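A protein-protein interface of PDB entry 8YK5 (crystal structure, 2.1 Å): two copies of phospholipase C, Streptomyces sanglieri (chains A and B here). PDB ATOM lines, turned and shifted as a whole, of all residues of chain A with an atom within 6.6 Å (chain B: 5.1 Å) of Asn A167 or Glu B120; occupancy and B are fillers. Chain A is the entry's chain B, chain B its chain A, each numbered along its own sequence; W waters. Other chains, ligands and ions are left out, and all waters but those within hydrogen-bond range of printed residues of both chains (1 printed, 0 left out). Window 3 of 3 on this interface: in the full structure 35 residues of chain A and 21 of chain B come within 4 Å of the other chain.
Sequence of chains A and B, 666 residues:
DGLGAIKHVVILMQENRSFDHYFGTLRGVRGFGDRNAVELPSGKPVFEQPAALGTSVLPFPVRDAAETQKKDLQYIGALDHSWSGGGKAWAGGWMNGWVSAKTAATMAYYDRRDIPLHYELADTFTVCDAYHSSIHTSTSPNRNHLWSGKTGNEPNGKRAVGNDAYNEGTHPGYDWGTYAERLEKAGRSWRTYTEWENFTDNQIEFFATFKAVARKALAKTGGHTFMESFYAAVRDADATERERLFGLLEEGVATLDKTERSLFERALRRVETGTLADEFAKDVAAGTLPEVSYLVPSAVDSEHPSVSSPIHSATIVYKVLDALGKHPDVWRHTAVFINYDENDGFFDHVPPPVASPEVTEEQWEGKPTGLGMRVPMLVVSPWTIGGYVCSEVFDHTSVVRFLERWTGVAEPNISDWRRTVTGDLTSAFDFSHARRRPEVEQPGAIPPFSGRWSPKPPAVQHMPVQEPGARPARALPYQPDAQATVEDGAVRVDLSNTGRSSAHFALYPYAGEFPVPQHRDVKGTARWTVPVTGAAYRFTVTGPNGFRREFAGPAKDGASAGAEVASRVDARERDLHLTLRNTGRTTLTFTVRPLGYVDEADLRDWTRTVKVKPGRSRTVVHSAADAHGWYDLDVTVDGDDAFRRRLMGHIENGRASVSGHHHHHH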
ATOM      1  N   ASN A 163     -16.008  -8.204   1.455  1.00  0.00           N
ATOM      2  CA  ASN A 163     -14.782  -7.713   0.906  1.00  0.00           C
ATOM      3  C   ASN A 163     -13.688  -8.727   0.745  1.00  0.00           C
ATOM      4  O   ASN A 163     -12.527  -8.396   0.816  1.00  0.00           O
ATOM      5  CB  ASN A 163     -14.221  -6.698   1.818  1.00  0.00           C
ATOM      6  CG  ASN A 163     -14.933  -5.429   1.814  1.00  0.00           C
ATOM      7  OD1 ASN A 163     -15.709  -5.064   1.000  1.00  0.00           O
ATOM      8  ND2 ASN A 163     -14.637  -4.727   2.793  1.00  0.00           N
ATOM      9  N   ASP A 164     -14.069  -9.952   0.484  1.00  0.00           N
ATOM     10  CA  ASP A 164     -13.101 -11.041   0.347  1.00  0.00           C
ATOM     11  C   ASP A 164     -12.001 -10.733  -0.668  1.00  0.00           C
ATOM     12  O   ASP A 164     -10.856 -11.158  -0.489  1.00  0.00           O
ATOM     13  CB  ASP A 164     -13.820 -12.332  -0.053  1.00  0.00           C
ATOM     14  CG  ASP A 164     -14.813 -12.791   0.993  1.00  0.00           C
ATOM     15  OD1 ASP A 164     -14.694 -13.936   1.476  1.00  0.00           O
ATOM     16  OD2 ASP A 164     -15.717 -12.004   1.340  1.00  0.00           O
ATOM     17  N   ALA A 165     -12.324  -9.996  -1.737  1.00  0.00           N
ATOM     18  CA  ALA A 165     -11.342  -9.721  -2.785  1.00  0.00           C
ATOM     19  C   ALA A 165     -10.143  -8.895  -2.301  1.00  0.00           C
ATOM     20  O   ALA A 165      -9.116  -8.866  -2.986  1.00  0.00           O
ATOM     21  CB  ALA A 165     -12.016  -9.009  -3.957  1.00  0.00           C
ATOM     22  N   TYR A 166     -10.240  -8.225  -1.146  1.00  0.00           N
ATOM     23  CA  TYR A 166      -9.123  -7.406  -0.678  1.00  0.00           C
ATOM     24  C   TYR A 166      -7.954  -8.249  -0.190  1.00  0.00           C
ATOM     25  O   TYR A 166      -6.858  -7.715   0.022  1.00  0.00           O
ATOM     26  CB  TYR A 166      -9.567  -6.473   0.449  1.00  0.00           C
ATOM     27  CG  TYR A 166     -10.581  -5.436   0.044  1.00  0.00           C
ATOM     28  CD1 TYR A 166     -11.207  -4.656   1.006  1.00  0.00           C
ATOM     29  CD2 TYR A 166     -10.912  -5.227  -1.298  1.00  0.00           C
ATOM     30  CE1 TYR A 166     -12.134  -3.713   0.663  1.00  0.00           C
ATOM     31  CE2 TYR A 166     -11.855  -4.289  -1.653  1.00  0.00           C
ATOM     32  CZ  TYR A 166     -12.458  -3.539  -0.658  1.00  0.00           C
ATOM     33  OH  TYR A 166     -13.374  -2.605  -0.980  1.00  0.00           O
ATOM     34  N   ASN A 167      -8.166  -9.543   0.017  1.00  0.00           N
ATOM     35  CA  ASN A 167      -7.076 -10.461   0.336  1.00  0.00           C
ATOM     36  C   ASN A 167      -6.444 -10.893  -0.990  1.00  0.00           C
ATOM     37  O   ASN A 167      -6.633 -12.005  -1.490  1.00  0.00           O
ATOM     38  CB  ASN A 167      -7.604 -11.630   1.155  1.00  0.00           C
ATOM     39  CG  ASN A 167      -6.520 -12.589   1.570  1.00  0.00           C
ATOM     40  OD1 ASN A 167      -5.330 -12.328   1.364  1.00  0.00           O
ATOM     41  ND2 ASN A 167      -6.922 -13.724   2.140  1.00  0.00           N
ATOM     42  N   GLU A 168      -5.691  -9.958  -1.574  1.00  0.00           N
ATOM     43  CA  GLU A 168      -5.354 -10.039  -2.990  1.00  0.00           C
ATOM     44  C   GLU A 168      -4.305 -11.092  -3.289  1.00  0.00           C
ATOM     45  O   GLU A 168      -4.246 -11.572  -4.427  1.00  0.00           O
ATOM     46  CB  GLU A 168      -4.874  -8.678  -3.501  1.00  0.00           C
ATOM     47  CG  GLU A 168      -5.941  -7.601  -3.434  1.00  0.00           C
ATOM     48  CD  GLU A 168      -5.358  -6.194  -3.443  1.00  0.00           C
ATOM     49  OE1 GLU A 168      -5.168  -5.603  -2.342  1.00  0.00           O
ATOM     50  OE2 GLU A 168      -5.083  -5.694  -4.558  1.00  0.00           O
ATOM     51  N   GLY A 169      -3.479 -11.457  -2.303  1.00  0.00           N
ATOM     52  CA  GLY A 169      -2.500 -12.509  -2.489  1.00  0.00           C
ATOM     53  C   GLY A 169      -3.064 -13.910  -2.452  1.00  0.00           C
ATOM     54  O   GLY A 169      -2.348 -14.863  -2.770  1.00  0.00           O
ATOM     55  N   THR A 170      -4.322 -14.059  -2.065  1.00  0.00           N
ATOM     56  CA  THR A 170      -4.963 -15.364  -2.010  1.00  0.00           C
ATOM     57  C   THR A 170      -6.193 -15.454  -2.896  1.00  0.00           C
ATOM     58  O   THR A 170      -6.343 -16.438  -3.629  1.00  0.00           O
ATOM     59  CB  THR A 170      -5.341 -15.715  -0.551  1.00  0.00           C
ATOM     60  OG1 THR A 170      -4.154 -15.795   0.261  1.00  0.00           O
ATOM     61  CG2 THR A 170      -6.092 -17.057  -0.487  1.00  0.00           C
ATOM     62  N   HIS A 171      -7.063 -14.448  -2.862  1.00  0.00           N
ATOM     63  CA  HIS A 171      -8.301 -14.471  -3.646  1.00  0.00           C
ATOM     64  C   HIS A 171      -7.977 -14.478  -5.144  1.00  0.00           C
ATOM     65  O   HIS A 171      -7.122 -13.700  -5.592  1.00  0.00           O
ATOM     66  CB  HIS A 171      -9.141 -13.246  -3.267  1.00  0.00           C
ATOM     67  CG  HIS A 171     -10.519 -13.221  -3.854  1.00  0.00           C
ATOM     68  ND1 HIS A 171     -10.795 -12.645  -5.077  1.00  0.00           N
ATOM     69  CD2 HIS A 171     -11.711 -13.631  -3.354  1.00  0.00           C
ATOM     70  CE1 HIS A 171     -12.091 -12.738  -5.323  1.00  0.00           C
ATOM     71  NE2 HIS A 171     -12.671 -13.326  -4.290  1.00  0.00           N
ATOM     72  N   PRO A 172      -8.610 -15.343  -5.945  1.00  0.00           N
ATOM     73  CA  PRO A 172      -8.241 -15.434  -7.365  1.00  0.00           C
ATOM     74  C   PRO A 172      -8.870 -14.375  -8.258  1.00  0.00           C
ATOM     75  O   PRO A 172      -8.545 -14.344  -9.451  1.00  0.00           O
ATOM     76  CB  PRO A 172      -8.746 -16.828  -7.759  1.00  0.00           C
ATOM     77  CG  PRO A 172      -9.950 -16.993  -6.918  1.00  0.00           C
ATOM     78  CD  PRO A 172      -9.606 -16.368  -5.583  1.00  0.00           C
ATOM     79  N   PHE A 206      -9.657  -6.343  -9.038  1.00  0.00           N
ATOM     80  CA  PHE A 206     -10.057  -7.617  -8.444  1.00  0.00           C
ATOM     81  C   PHE A 206     -10.788  -8.527  -9.419  1.00  0.00           C
ATOM     82  O   PHE A 206     -11.399  -9.509  -8.989  1.00  0.00           O
ATOM     83  CB  PHE A 206     -10.927  -7.375  -7.205  1.00  0.00           C
ATOM     84  CG  PHE A 206     -10.381  -6.314  -6.314  1.00  0.00           C
ATOM     85  CD1 PHE A 206      -9.097  -6.437  -5.784  1.00  0.00           C
ATOM     86  CD2 PHE A 206     -11.116  -5.159  -6.059  1.00  0.00           C
ATOM     87  CE1 PHE A 206      -8.553  -5.435  -5.000  1.00  0.00           C
ATOM     88  CE2 PHE A 206     -10.589  -4.155  -5.262  1.00  0.00           C
ATOM     89  CZ  PHE A 206      -9.303  -4.294  -4.726  1.00  0.00           C
ATOM     90  N   LYS A 211      -6.160  -9.256 -12.733  1.00  0.00           N
ATOM     91  CA  LYS A 211      -5.181  -9.930 -11.885  1.00  0.00           C
ATOM     92  C   LYS A 211      -4.128 -10.641 -12.732  1.00  0.00           C
ATOM     93  O   LYS A 211      -2.947 -10.683 -12.360  1.00  0.00           O
ATOM     94  CB  LYS A 211      -5.872 -10.914 -10.940  1.00  0.00           C
ATOM     95  CG  LYS A 211      -6.846 -10.255  -9.979  1.00  0.00           C
ATOM     96  CD  LYS A 211      -7.142 -11.128  -8.753  1.00  0.00           C
ATOM     97  CE  LYS A 211      -5.921 -11.243  -7.868  1.00  0.00           C
ATOM     98  NZ  LYS A 211      -6.265 -11.088  -6.463  1.00  0.00           N
ATOM     99  N   PHE A 226       0.409  -8.711  -7.254  1.00  0.00           N
ATOM    100  CA  PHE A 226      -0.703  -7.799  -7.473  1.00  0.00           C
ATOM    101  C   PHE A 226      -0.182  -6.387  -7.270  1.00  0.00           C
ATOM    102  O   PHE A 226       0.794  -6.175  -6.539  1.00  0.00           O
ATOM    103  CB  PHE A 226      -1.916  -8.087  -6.538  1.00  0.00           C
ATOM    104  CG  PHE A 226      -1.585  -8.101  -5.047  1.00  0.00           C
ATOM    105  CD1 PHE A 226      -1.057  -9.237  -4.436  1.00  0.00           C
ATOM    106  CD2 PHE A 226      -1.856  -6.992  -4.258  1.00  0.00           C
ATOM    107  CE1 PHE A 226      -0.779  -9.255  -3.074  1.00  0.00           C
ATOM    108  CE2 PHE A 226      -1.587  -6.999  -2.902  1.00  0.00           C
ATOM    109  CZ  PHE A 226      -1.036  -8.134  -2.304  1.00  0.00           C
ATOM    110  N   ARG B  27       1.070 -19.491   2.824  1.00  0.00           N
ATOM    111  CA  ARG B  27       1.939 -18.700   1.954  1.00  0.00           C
ATOM    112  C   ARG B  27       2.789 -17.719   2.757  1.00  0.00           C
ATOM    113  O   ARG B  27       2.297 -17.051   3.674  1.00  0.00           O
ATOM    114  CB  ARG B  27       1.108 -17.932   0.926  1.00  0.00           C
ATOM    115  CG  ARG B  27       1.886 -16.793   0.249  1.00  0.00           C
ATOM    116  CD  ARG B  27       1.083 -16.134  -0.870  1.00  0.00           C
ATOM    117  NE  ARG B  27      -0.223 -15.699  -0.391  1.00  0.00           N
ATOM    118  CZ  ARG B  27      -0.458 -14.523   0.185  1.00  0.00           C
ATOM    119  NH1 ARG B  27       0.540 -13.662   0.340  1.00  0.00           N
ATOM    120  NH2 ARG B  27      -1.690 -14.221   0.610  1.00  0.00           N
ATOM    121  N   ARG B 112      -5.482 -24.800   4.682  1.00  0.00           N
ATOM    122  CA  ARG B 112      -6.451 -23.712   4.616  1.00  0.00           C
ATOM    123  C   ARG B 112      -7.879 -24.217   4.457  1.00  0.00           C
ATOM    124  O   ARG B 112      -8.815 -23.571   4.943  1.00  0.00           O
ATOM    125  CB  ARG B 112      -6.088 -22.757   3.475  1.00  0.00           C
ATOM    126  CG  ARG B 112      -7.082 -21.605   3.275  1.00  0.00           C
ATOM    127  CD  ARG B 112      -6.708 -20.753   2.061  1.00  0.00           C
ATOM    128  NE  ARG B 112      -5.364 -20.196   2.178  1.00  0.00           N
ATOM    129  CZ  ARG B 112      -5.103 -18.999   2.690  1.00  0.00           C
ATOM    130  NH1 ARG B 112      -6.099 -18.233   3.135  1.00  0.00           N
ATOM    131  NH2 ARG B 112      -3.850 -18.565   2.742  1.00  0.00           N
ATOM    132  N   PRO B 116     -10.093 -22.488   7.849  1.00  0.00           N
ATOM    133  CA  PRO B 116     -10.083 -21.264   7.041  1.00  0.00           C
ATOM    134  C   PRO B 116     -10.062 -19.992   7.871  1.00  0.00           C
ATOM    135  O   PRO B 116      -9.433 -19.018   7.447  1.00  0.00           O
ATOM    136  CB  PRO B 116     -11.360 -21.390   6.201  1.00  0.00           C
ATOM    137  CG  PRO B 116     -12.264 -22.218   7.034  1.00  0.00           C
ATOM    138  CD  PRO B 116     -11.377 -23.205   7.748  1.00  0.00           C
ATOM    139  N   LEU B 117     -10.701 -19.955   9.044  1.00  0.00           N
ATOM    140  CA  LEU B 117     -10.621 -18.742   9.858  1.00  0.00           C
ATOM    141  C   LEU B 117      -9.187 -18.465  10.293  1.00  0.00           C
ATOM    142  O   LEU B 117      -8.746 -17.307  10.313  1.00  0.00           O
ATOM    143  CB  LEU B 117     -11.526 -18.834  11.088  1.00  0.00           C
ATOM    144  CG  LEU B 117     -11.302 -17.573  11.945  1.00  0.00           C
ATOM    145  CD1 LEU B 117     -11.844 -16.425  11.157  1.00  0.00           C
ATOM    146  CD2 LEU B 117     -11.909 -17.564  13.338  1.00  0.00           C
ATOM    147  N   HIS B 118      -8.441 -19.516  10.642  1.00  0.00           N
ATOM    148  CA  HIS B 118      -7.049 -19.324  11.036  1.00  0.00           C
ATOM    149  C   HIS B 118      -6.241 -18.713   9.890  1.00  0.00           C
ATOM    150  O   HIS B 118      -5.455 -17.780  10.091  1.00  0.00           O
ATOM    151  CB  HIS B 118      -6.435 -20.659  11.475  1.00  0.00           C
ATOM    152  CG  HIS B 118      -7.082 -21.274  12.682  1.00  0.00           C
ATOM    153  ND1 HIS B 118      -8.430 -21.572  12.741  1.00  0.00           N
ATOM    154  CD2 HIS B 118      -6.555 -21.676  13.865  1.00  0.00           C
ATOM    155  CE1 HIS B 118      -8.708 -22.107  13.917  1.00  0.00           C
ATOM    156  NE2 HIS B 118      -7.587 -22.188  14.615  1.00  0.00           N
ATOM    157  N   TYR B 119      -6.421 -19.239   8.678  1.00  0.00           N
ATOM    158  CA  TYR B 119      -5.646 -18.765   7.540  1.00  0.00           C
ATOM    159  C   TYR B 119      -6.059 -17.356   7.145  1.00  0.00           C
ATOM    160  O   TYR B 119      -5.205 -16.513   6.833  1.00  0.00           O
ATOM    161  CB  TYR B 119      -5.798 -19.732   6.366  1.00  0.00           C
ATOM    162  CG  TYR B 119      -4.794 -20.863   6.414  1.00  0.00           C
ATOM    163  CD1 TYR B 119      -3.812 -20.980   5.439  1.00  0.00           C
ATOM    164  CD2 TYR B 119      -4.824 -21.820   7.443  1.00  0.00           C
ATOM    165  CE1 TYR B 119      -2.877 -22.011   5.481  1.00  0.00           C
ATOM    166  CE2 TYR B 119      -3.890 -22.861   7.489  1.00  0.00           C
ATOM    167  CZ  TYR B 119      -2.915 -22.940   6.505  1.00  0.00           C
ATOM    168  OH  TYR B 119      -1.980 -23.943   6.525  1.00  0.00           O
ATOM    169  N   GLU B 120      -7.359 -17.074   7.170  1.00  0.00           N
ATOM    170  CA  GLU B 120      -7.826 -15.745   6.806  1.00  0.00           C
ATOM    171  C   GLU B 120      -7.324 -14.690   7.784  1.00  0.00           C
ATOM    172  O   GLU B 120      -7.077 -13.541   7.389  1.00  0.00           O
ATOM    173  CB  GLU B 120      -9.354 -15.737   6.718  1.00  0.00           C
ATOM    174  CG  GLU B 120      -9.938 -14.669   5.723  1.00  0.00           C
ATOM    175  CD  GLU B 120      -9.562 -14.900   4.223  1.00  0.00           C
ATOM    176  OE1 GLU B 120      -9.201 -16.043   3.839  1.00  0.00           O
ATOM    177  OE2 GLU B 120      -9.637 -13.926   3.419  1.00  0.00           O
ATOM    178  N   LEU B 121      -7.139 -15.064   9.053  1.00  0.00           N
ATOM    179  CA  LEU B 121      -6.652 -14.106  10.040  1.00  0.00           C
ATOM    180  C   LEU B 121      -5.193 -13.762   9.795  1.00  0.00           C
ATOM    181  O   LEU B 121      -4.782 -12.600   9.934  1.00  0.00           O
ATOM    182  CB  LEU B 121      -6.824 -14.668  11.447  1.00  0.00           C
ATOM    183  CG  LEU B 121      -8.145 -14.431  12.161  1.00  0.00           C
ATOM    184  CD1 LEU B 121      -8.035 -15.053  13.530  1.00  0.00           C
ATOM    185  CD2 LEU B 121      -8.477 -12.953  12.273  1.00  0.00           C
ATOM    186  N   ALA B 122      -4.387 -14.766   9.454  1.00  0.00           N
ATOM    187  CA  ALA B 122      -2.996 -14.514   9.101  1.00  0.00           C
ATOM    188  C   ALA B 122      -2.881 -13.671   7.831  1.00  0.00           C
ATOM    189  O   ALA B 122      -1.962 -12.847   7.714  1.00  0.00           O
ATOM    190  CB  ALA B 122      -2.265 -15.844   8.931  1.00  0.00           C
ATOM    191  N   ASP B 123      -3.797 -13.877   6.867  1.00  0.00           N
ATOM    192  CA  ASP B 123      -3.793 -13.151   5.599  1.00  0.00           C
ATOM    193  C   ASP B 123      -4.249 -11.707   5.755  1.00  0.00           C
ATOM    194  O   ASP B 123      -3.963 -10.871   4.890  1.00  0.00           O
ATOM    195  CB  ASP B 123      -4.733 -13.819   4.586  1.00  0.00           C
ATOM    196  CG  ASP B 123      -4.099 -14.976   3.834  1.00  0.00           C
ATOM    197  OD1 ASP B 123      -2.880 -15.219   3.971  1.00  0.00           O
ATOM    198  OD2 ASP B 123      -4.844 -15.644   3.074  1.00  0.00           O
ATOM    199  N   THR B 124      -4.988 -11.411   6.814  1.00  0.00           N
ATOM    200  CA  THR B 124      -5.568 -10.097   7.034  1.00  0.00           C
ATOM    201  C   THR B 124      -4.748  -9.248   7.986  1.00  0.00           C
ATOM    202  O   THR B 124      -4.700  -8.020   7.844  1.00  0.00           O
ATOM    203  CB  THR B 124      -6.983 -10.261   7.602  1.00  0.00           C
ATOM    204  OG1 THR B 124      -7.760 -11.040   6.688  1.00  0.00           O
ATOM    205  CG2 THR B 124      -7.647  -8.934   7.773  1.00  0.00           C
ATOM    206  N   PHE B 125      -4.101  -9.871   8.958  1.00  0.00           N
ATOM    207  CA  PHE B 125      -3.437  -9.104   9.993  1.00  0.00           C
ATOM    208  C   PHE B 125      -1.945  -9.390   9.910  1.00  0.00           C
ATOM    209  O   PHE B 125      -1.371  -9.273   8.823  1.00  0.00           O
ATOM    210  CB  PHE B 125      -4.070  -9.439  11.355  1.00  0.00           C
ATOM    211  CG  PHE B 125      -5.468  -8.895  11.490  1.00  0.00           C
ATOM    212  CD1 PHE B 125      -5.676  -7.553  11.820  1.00  0.00           C
ATOM    213  CD2 PHE B 125      -6.571  -9.700  11.251  1.00  0.00           C
ATOM    214  CE1 PHE B 125      -6.970  -7.041  11.950  1.00  0.00           C
ATOM    215  CE2 PHE B 125      -7.869  -9.194  11.354  1.00  0.00           C
ATOM    216  CZ  PHE B 125      -8.072  -7.861  11.703  1.00  0.00           C
HETATM  217  O   HOH W   1      -2.269 -18.060  -0.844  1.00  0.00           O
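The side-chain carboxylate (OD1) of Asp B123 is in salt-bridge range of the guanidinium group (NH2) of Arg B27 (3.7 Å). The guanidinium group (NH1) of Arg B112 is in salt-bridge range of the side-chain carboxylate (OE1) of Glu B120 (3.9 Å). The side-chain carboxylate (OD2) of Asp B123 is in salt-bridge range of the guanidinium group (NH1) of Arg B112, at 2.9 Å. OG1 of Thr B124 sits at hydrogen-bond distance from O of Glu B120, 2.7 Å away.
No position is printed for both chains. Of the 6 pairs that touch across the chains among the printed residues, none has its exchanged pair printed and touching as well.
Among the printed residues, pairs that only touch across the chains: Thr A170 with Arg B112.
Asn A167 touches just these residues of chain B: Glu B120 and Asp B123. Of the printed residues of chain B, Gly A169 touches Arg B27. Printed residues of chain B within 4 Å of Thr A170: Arg B27, Arg B112 and Asp B123. Printed residues of chain A within 4 Å of Arg B27: Gly A169 and Thr A170. Of the printed residues of chain A, Arg B112 touches Thr A170. Of chain A, only Asn A167 (3.0 Å) comes within 4 Å of Glu B120. Ala B122 touches none of the printed residues of chain A. Of the printed residues of chain A, Asp B123 touches Asn A167 and Thr A170. The nearest residue of chain A that does not touch Glu B120 is Asp A164 (4.9 Å). The nearest printed residue of chain B that does not touch Gly A169 is Asp B123 (6.1 Å).
Printed residues of chain A that touch a printed residue of chain B: Asn A167, Gly A169 and Thr A170. Of the 12 printed residues of chain B, 4 touch a printed residue of chain A. Among the printed residues, 6 pairs touch across the chains.
Water W1 lies within hydrogen-bond range of OG1 of Thr A170 (3.1 Å) and NE of Arg B27 (3.2 Å).
The guanidinium group of Arg B27 lies within hydrogen-bond range of the backbone carbonyl oxygen of Gly A169, at 3.3 Å. The guanidinium group of Arg B27 lies within hydrogen-bond range of the side-chain hydroxyl of Thr A170 (2.9 Å). The side-chain carboxylate of Glu B120 is in hydrogen-bond range of the side-chain amide nitrogen of Asn A167 (3.0 Å). The side-chain carboxylate of Asp B123 is in hydrogen-bond range of the side-chain amide nitrogen of Asn A167, at 3.0 Å. OD2 of Asp B123 sits at hydrogen-bond distance from OG1 of Thr A170, 2.9 Å away.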
